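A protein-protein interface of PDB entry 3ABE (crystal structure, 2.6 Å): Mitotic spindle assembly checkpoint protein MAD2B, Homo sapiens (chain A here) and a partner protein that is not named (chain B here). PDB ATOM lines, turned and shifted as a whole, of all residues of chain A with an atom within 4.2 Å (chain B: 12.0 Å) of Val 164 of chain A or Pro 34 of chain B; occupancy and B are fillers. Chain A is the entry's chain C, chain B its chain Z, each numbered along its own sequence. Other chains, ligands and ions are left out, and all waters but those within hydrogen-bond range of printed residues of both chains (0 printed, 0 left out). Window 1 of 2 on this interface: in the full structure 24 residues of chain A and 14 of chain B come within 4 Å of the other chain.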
ATOM      1  N   TYR A  79     -19.633 -18.617  11.268  1.00  0.00           N
ATOM      2  CA  TYR A  79     -18.879 -19.751  10.872  1.00  0.00           C
ATOM      3  C   TYR A  79     -19.651 -20.986  11.235  1.00  0.00           C
ATOM      4  O   TYR A  79     -19.724 -21.921  10.454  1.00  0.00           O
ATOM      5  CB  TYR A  79     -17.529 -19.738  11.559  1.00  0.00           C
ATOM      6  CG  TYR A  79     -16.650 -20.886  11.175  1.00  0.00           C
ATOM      7  CD1 TYR A  79     -15.865 -20.832  10.057  1.00  0.00           C
ATOM      8  CD2 TYR A  79     -16.614 -22.033  11.949  1.00  0.00           C
ATOM      9  CE1 TYR A  79     -15.065 -21.911   9.713  1.00  0.00           C
ATOM     10  CE2 TYR A  79     -15.821 -23.100  11.632  1.00  0.00           C
ATOM     11  CZ  TYR A  79     -15.048 -23.044  10.528  1.00  0.00           C
ATOM     12  OH  TYR A  79     -14.277 -24.137  10.228  1.00  0.00           O
ATOM     13  N   THR A  83     -21.557 -23.761   9.045  1.00  0.00           N
ATOM     14  CA  THR A  83     -21.171 -25.161   9.110  1.00  0.00           C
ATOM     15  C   THR A  83     -22.425 -26.001   9.213  1.00  0.00           C
ATOM     16  O   THR A  83     -22.642 -26.916   8.405  1.00  0.00           O
ATOM     17  CB  THR A  83     -20.216 -25.400  10.296  1.00  0.00           C
ATOM     18  OG1 THR A  83     -18.957 -24.786   9.981  1.00  0.00           O
ATOM     19  CG2 THR A  83     -19.977 -26.894  10.562  1.00  0.00           C
ATOM     20  N   VAL A  99     -21.226 -36.227  13.909  1.00  0.00           N
ATOM     21  CA  VAL A  99     -20.646 -34.911  13.899  1.00  0.00           C
ATOM     22  C   VAL A  99     -19.660 -34.740  15.042  1.00  0.00           C
ATOM     23  O   VAL A  99     -20.031 -34.798  16.203  1.00  0.00           O
ATOM     24  CB  VAL A  99     -21.657 -33.840  14.054  1.00  0.00           C
ATOM     25  CG1 VAL A  99     -20.896 -32.530  14.214  1.00  0.00           C
ATOM     26  CG2 VAL A  99     -22.615 -33.854  12.863  1.00  0.00           C
ATOM     27  N   VAL A 100     -18.400 -34.521  14.690  1.00  0.00           N
ATOM     28  CA  VAL A 100     -17.330 -34.410  15.659  1.00  0.00           C
ATOM     29  C   VAL A 100     -16.809 -32.984  15.765  1.00  0.00           C
ATOM     30  O   VAL A 100     -16.436 -32.374  14.773  1.00  0.00           O
ATOM     31  CB  VAL A 100     -16.171 -35.316  15.270  1.00  0.00           C
ATOM     32  CG1 VAL A 100     -15.072 -35.257  16.299  1.00  0.00           C
ATOM     33  CG2 VAL A 100     -16.663 -36.710  15.118  1.00  0.00           C
ATOM     34  N   THR A 163     -12.525 -27.213  14.767  1.00  0.00           N
ATOM     35  CA  THR A 163     -12.814 -27.660  13.443  1.00  0.00           C
ATOM     36  C   THR A 163     -13.998 -28.569  13.645  1.00  0.00           C
ATOM     37  O   THR A 163     -14.263 -28.982  14.770  1.00  0.00           O
ATOM     38  CB  THR A 163     -11.636 -28.459  12.945  1.00  0.00           C
ATOM     39  OG1 THR A 163     -11.416 -28.174  11.569  1.00  0.00           O
ATOM     40  CG2 THR A 163     -11.863 -29.957  13.158  1.00  0.00           C
ATOM     41  N   VAL A 164     -14.720 -28.893  12.591  1.00  0.00           N
ATOM     42  CA  VAL A 164     -15.862 -29.787  12.731  1.00  0.00           C
ATOM     43  C   VAL A 164     -15.758 -30.761  11.625  1.00  0.00           C
ATOM     44  O   VAL A 164     -15.519 -30.374  10.503  1.00  0.00           O
ATOM     45  CB  VAL A 164     -17.167 -29.019  12.558  1.00  0.00           C
ATOM     46  CG1 VAL A 164     -18.374 -29.987  12.434  1.00  0.00           C
ATOM     47  CG2 VAL A 164     -17.350 -27.996  13.704  1.00  0.00           C
ATOM     48  N   LEU A 165     -15.897 -32.032  11.930  1.00  0.00           N
ATOM     49  CA  LEU A 165     -15.853 -33.061  10.908  1.00  0.00           C
ATOM     50  C   LEU A 165     -17.182 -33.773  10.874  1.00  0.00           C
ATOM     51  O   LEU A 165     -17.804 -33.936  11.910  1.00  0.00           O
ATOM     52  CB  LEU A 165     -14.784 -34.084  11.247  1.00  0.00           C
ATOM     53  CG  LEU A 165     -13.375 -33.631  11.586  1.00  0.00           C
ATOM     54  CD1 LEU A 165     -12.522 -34.910  11.744  1.00  0.00           C
ATOM     55  CD2 LEU A 165     -12.810 -32.785  10.516  1.00  0.00           C
ATOM     56  N   PHE A 185     -18.913 -20.916   1.492  1.00  0.00           N
ATOM     57  CA  PHE A 185     -18.539 -21.821   2.601  1.00  0.00           C
ATOM     58  C   PHE A 185     -18.313 -23.282   2.156  1.00  0.00           C
ATOM     59  O   PHE A 185     -19.163 -24.149   2.319  1.00  0.00           O
ATOM     60  CB  PHE A 185     -19.529 -21.779   3.736  1.00  0.00           C
ATOM     61  CG  PHE A 185     -18.958 -22.302   5.011  1.00  0.00           C
ATOM     62  CD1 PHE A 185     -18.077 -21.532   5.753  1.00  0.00           C
ATOM     63  CD2 PHE A 185     -19.219 -23.572   5.434  1.00  0.00           C
ATOM     64  CE1 PHE A 185     -17.547 -21.998   6.880  1.00  0.00           C
ATOM     65  CE2 PHE A 185     -18.688 -23.997   6.597  1.00  0.00           C
ATOM     66  CZ  PHE A 185     -17.877 -23.205   7.313  1.00  0.00           C
ATOM     67  N   PRO A 186     -17.160 -23.543   1.558  1.00  0.00           N
ATOM     68  CA  PRO A 186     -16.959 -24.834   0.921  1.00  0.00           C
ATOM     69  C   PRO A 186     -16.451 -25.921   1.861  1.00  0.00           C
ATOM     70  O   PRO A 186     -15.831 -25.623   2.887  1.00  0.00           O
ATOM     71  CB  PRO A 186     -15.914 -24.511  -0.144  1.00  0.00           C
ATOM     72  CG  PRO A 186     -15.692 -22.943  -0.019  1.00  0.00           C
ATOM     73  CD  PRO A 186     -16.029 -22.632   1.315  1.00  0.00           C
ATOM     74  N   TRP A 187     -16.738 -27.165   1.509  1.00  0.00           N
ATOM     75  CA  TRP A 187     -16.275 -28.284   2.314  1.00  0.00           C
ATOM     76  C   TRP A 187     -15.408 -29.126   1.485  1.00  0.00           C
ATOM     77  O   TRP A 187     -15.714 -29.318   0.339  1.00  0.00           O
ATOM     78  CB  TRP A 187     -17.412 -29.179   2.780  1.00  0.00           C
ATOM     79  CG  TRP A 187     -18.292 -28.572   3.721  1.00  0.00           C
ATOM     80  CD1 TRP A 187     -19.162 -27.537   3.495  1.00  0.00           C
ATOM     81  CD2 TRP A 187     -18.444 -28.954   5.071  1.00  0.00           C
ATOM     82  NE1 TRP A 187     -19.857 -27.243   4.666  1.00  0.00           N
ATOM     83  CE2 TRP A 187     -19.431 -28.096   5.646  1.00  0.00           C
ATOM     84  CE3 TRP A 187     -17.835 -29.921   5.865  1.00  0.00           C
ATOM     85  CZ2 TRP A 187     -19.825 -28.196   6.933  1.00  0.00           C
ATOM     86  CZ3 TRP A 187     -18.217 -30.028   7.166  1.00  0.00           C
ATOM     87  CH2 TRP A 187     -19.218 -29.180   7.697  1.00  0.00           C
ATOM     88  N   ASN B  30     -15.057 -41.487   4.819  1.00  0.00           N
ATOM     89  CA  ASN B  30     -16.419 -40.881   4.972  1.00  0.00           C
ATOM     90  C   ASN B  30     -16.536 -39.465   5.607  1.00  0.00           C
ATOM     91  O   ASN B  30     -17.531 -39.165   6.253  1.00  0.00           O
ATOM     92  CB  ASN B  30     -17.396 -41.856   5.691  1.00  0.00           C
ATOM     93  CG  ASN B  30     -16.728 -42.717   6.782  1.00  0.00           C
ATOM     94  OD1 ASN B  30     -15.956 -43.654   6.469  1.00  0.00           O
ATOM     95  ND2 ASN B  30     -17.084 -42.457   8.063  1.00  0.00           N
ATOM     96  N   ILE B  31     -15.564 -38.582   5.380  1.00  0.00           N
ATOM     97  CA  ILE B  31     -15.303 -37.529   6.344  1.00  0.00           C
ATOM     98  C   ILE B  31     -15.118 -36.113   5.732  1.00  0.00           C
ATOM     99  O   ILE B  31     -14.076 -35.833   5.138  1.00  0.00           O
ATOM    100  CB  ILE B  31     -14.074 -37.923   7.195  1.00  0.00           C
ATOM    101  CG1 ILE B  31     -14.235 -39.344   7.775  1.00  0.00           C
ATOM    102  CG2 ILE B  31     -13.885 -36.993   8.349  1.00  0.00           C
ATOM    103  CD1 ILE B  31     -12.961 -39.944   8.326  1.00  0.00           C
ATOM    104  N   LEU B  32     -16.116 -35.235   5.912  1.00  0.00           N
ATOM    105  CA  LEU B  32     -16.096 -33.879   5.351  1.00  0.00           C
ATOM    106  C   LEU B  32     -15.818 -32.755   6.352  1.00  0.00           C
ATOM    107  O   LEU B  32     -16.251 -32.771   7.487  1.00  0.00           O
ATOM    108  CB  LEU B  32     -17.442 -33.552   4.703  1.00  0.00           C
ATOM    109  CG  LEU B  32     -17.855 -34.365   3.481  1.00  0.00           C
ATOM    110  CD1 LEU B  32     -17.207 -35.735   3.570  1.00  0.00           C
ATOM    111  CD2 LEU B  32     -19.391 -34.439   3.428  1.00  0.00           C
ATOM    112  N   LYS B  33     -15.127 -31.735   5.903  1.00  0.00           N
ATOM    113  CA  LYS B  33     -14.733 -30.686   6.794  1.00  0.00           C
ATOM    114  C   LYS B  33     -14.832 -29.391   6.025  1.00  0.00           C
ATOM    115  O   LYS B  33     -14.654 -29.381   4.798  1.00  0.00           O
ATOM    116  CB  LYS B  33     -13.320 -30.972   7.258  1.00  0.00           C
ATOM    117  CG  LYS B  33     -12.461 -29.828   7.759  1.00  0.00           C
ATOM    118  CD  LYS B  33     -11.010 -30.240   7.563  1.00  0.00           C
ATOM    119  CE  LYS B  33     -10.063 -29.106   7.780  1.00  0.00           C
ATOM    120  NZ  LYS B  33      -8.673 -29.617   7.642  1.00  0.00           N
ATOM    121  N   PRO B  34     -15.131 -28.298   6.731  1.00  0.00           N
ATOM    122  CA  PRO B  34     -15.177 -27.071   5.985  1.00  0.00           C
ATOM    123  C   PRO B  34     -13.771 -26.693   5.616  1.00  0.00           C
ATOM    124  O   PRO B  34     -12.868 -26.810   6.435  1.00  0.00           O
ATOM    125  CB  PRO B  34     -15.811 -26.058   6.960  1.00  0.00           C
ATOM    126  CG  PRO B  34     -16.213 -26.823   8.164  1.00  0.00           C
ATOM    127  CD  PRO B  34     -15.409 -28.104   8.158  1.00  0.00           C
ATOM    128  N   LEU B  35     -13.603 -26.282   4.364  1.00  0.00           N
ATOM    129  CA  LEU B  35     -12.366 -25.738   3.851  1.00  0.00           C
ATOM    130  C   LEU B  35     -11.831 -24.626   4.718  1.00  0.00           C
ATOM    131  O   LEU B  35     -10.631 -24.477   4.907  1.00  0.00           O
ATOM    132  CB  LEU B  35     -12.622 -25.140   2.474  1.00  0.00           C
ATOM    133  CG  LEU B  35     -11.382 -24.524   1.820  1.00  0.00           C
ATOM    134  CD1 LEU B  35     -10.253 -25.545   1.766  1.00  0.00           C
ATOM    135  CD2 LEU B  35     -11.705 -23.993   0.454  1.00  0.00           C
ATOM    136  N   MET B  36     -12.741 -23.818   5.217  1.00  0.00           N
ATOM    137  CA  MET B  36     -12.362 -22.631   5.905  1.00  0.00           C
ATOM    138  C   MET B  36     -12.166 -22.875   7.370  1.00  0.00           C
ATOM    139  O   MET B  36     -12.949 -23.604   7.988  1.00  0.00           O
ATOM    140  CB  MET B  36     -13.482 -21.635   5.794  1.00  0.00           C
ATOM    141  CG  MET B  36     -13.023 -20.325   5.401  1.00  0.00           C
ATOM    142  SD  MET B  36     -13.437 -20.171   3.694  1.00  0.00           S
ATOM    143  CE  MET B  36     -11.869 -19.512   3.064  1.00  0.00           C
ATOM    144  N   SER B  37     -11.167 -22.201   7.932  1.00  0.00           N
ATOM    145  CA  SER B  37     -10.960 -22.161   9.361  1.00  0.00           C
ATOM    146  C   SER B  37     -11.713 -21.023  10.043  1.00  0.00           C
ATOM    147  O   SER B  37     -12.037 -19.979   9.406  1.00  0.00           O
ATOM    148  CB  SER B  37      -9.491 -21.991   9.642  1.00  0.00           C
ATOM    149  OG  SER B  37      -8.774 -23.035   9.003  1.00  0.00           O
ATOM    150  N   PRO B  38     -12.020 -21.219  11.338  1.00  0.00           N
ATOM    151  CA  PRO B  38     -12.662 -20.173  12.104  1.00  0.00           C
ATOM    152  C   PRO B  38     -11.705 -19.102  12.539  1.00  0.00           C
ATOM    153  O   PRO B  38     -10.488 -19.344  12.583  1.00  0.00           O
ATOM    154  CB  PRO B  38     -13.174 -20.917  13.320  1.00  0.00           C
ATOM    155  CG  PRO B  38     -12.217 -22.077  13.476  1.00  0.00           C
ATOM    156  CD  PRO B  38     -11.884 -22.464  12.110  1.00  0.00           C
ATOM    157  N   PRO B  39     -12.245 -17.909  12.856  1.00  0.00           N
ATOM    158  CA  PRO B  39     -11.528 -16.773  13.408  1.00  0.00           C
ATOM    159  C   PRO B  39     -10.573 -17.197  14.490  1.00  0.00           C
ATOM    160  O   PRO B  39     -10.962 -17.962  15.364  1.00  0.00           O
ATOM    161  CB  PRO B  39     -12.640 -15.936  14.028  1.00  0.00           C
ATOM    162  CG  PRO B  39     -13.925 -16.690  13.770  1.00  0.00           C
ATOM    163  CD  PRO B  39     -13.657 -17.579  12.656  1.00  0.00           C
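The backbone carbonyl oxygen (O) of Met 36 of chain B sits at hydrogen-bond distance from the side-chain hydroxyl (OH) of Tyr 79 of chain A (2.7 Å). The backbone carbonyl oxygen (O) of Pro 186 of chain A sits at hydrogen-bond distance from the backbone NH (N) of Leu 35 of chain B (2.8 Å).
Printed residues of chain A that touch a printed residue of chain B: Tyr 79, Thr 83, Val 164, Leu 165, Phe 185, Pro 186 and Trp 187. Along chain A the printed residues that touch a printed residue of chain B span positions 79 to 187. Of the 10 printed residues of chain B, 7 touch a printed residue of chain A. Printed residues of chain B that touch a printed residue of chain A: Leu 32, Lys 33, Pro 34, Leu 35, Met 36, Ser 37 and Pro 38. Hydrophobic or aromatic side chains of chain B within 4 Å of the printed part of chain A: Leu 32, Pro 34, Leu 35 and Pro 38. Among the printed residues, 17 pairs touch across the chains.
Val 164 of chain A touches just these residues of chain B: Leu 32, Lys 33 and Pro 34. Of chain A, only Tyr 79, Thr 83, Val 164, Phe 185, Pro 186 and Trp 187 come within 4 Å of Pro 34 of chain B. Of chain B, only Pro 34 (3.9 Å) comes within 4 Å of Thr 83 of chain A. No residue of chain B comes within 4 Å of Val 99 of chain A. No residue of chain B comes within 4 Å of Val 100 of chain A. Pro 186 of chain A touches just these residues of chain B: Pro 34 and Leu 35. Of chain B, only Leu 32 (3.4 Å), Lys 33 (3.1 Å), Pro 34 (3.3 Å) and Leu 35 (3.9 Å) come within 4 Å of Trp 187 of chain A. Of the printed residues of chain A, Leu 32 of chain B touches Val 164, Leu 165 and Trp 187. Of the printed residues of chain A, Met 36 of chain B touches Tyr 79. Asn 30 of chain B touches none of the printed residues of chain A. Pro 39 of chain B touches none of the printed residues of chain A. The nearest residue of chain B that does not touch Val 164 of chain A is Pro 38 of chain B (7.0 Å). The nearest printed residue of chain A that does not touch Pro 34 of chain B is Thr 163 of chain A (5.3 Å). The nearest printed residue of chain B that does not touch Tyr 79 of chain A is Pro 39 of chain B (4.6 Å).
O of Tyr 79 of chain A sits at hydrogen-bond distance from OG1 of Thr 83 of chain A. N of Val 100 of chain A is in hydrogen-bond range of O of Leu 165 of chain A (2.9 Å).
Pro 34 of chain B touches Tyr 79 of chain A. CE1 of Tyr 79 of chain A touches C of Ser 37 of chain B, 3.5 Å away. OG1 of Thr 83 of chain A touches CG of Pro 34 of chain B (3.9 Å). Val 164 of chain A touches Leu 32 of chain B (O to O, 3.9 Å). Val 164 of chain A touches Pro 34 of chain B. Leu 32 of chain B touches Leu 165 of chain A (O to CA, 3.5 Å). Lys 33 of chain B touches Leu 165 of chain A. Trp 187 of chain A touches Lys 33 of chain B (CE3 to C, 3.1 Å). Pro 34 of chain B touches Trp 187 of chain A. N of Leu 35 of chain B touches CA of Trp 187 of chain A, at 3.9 Å.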
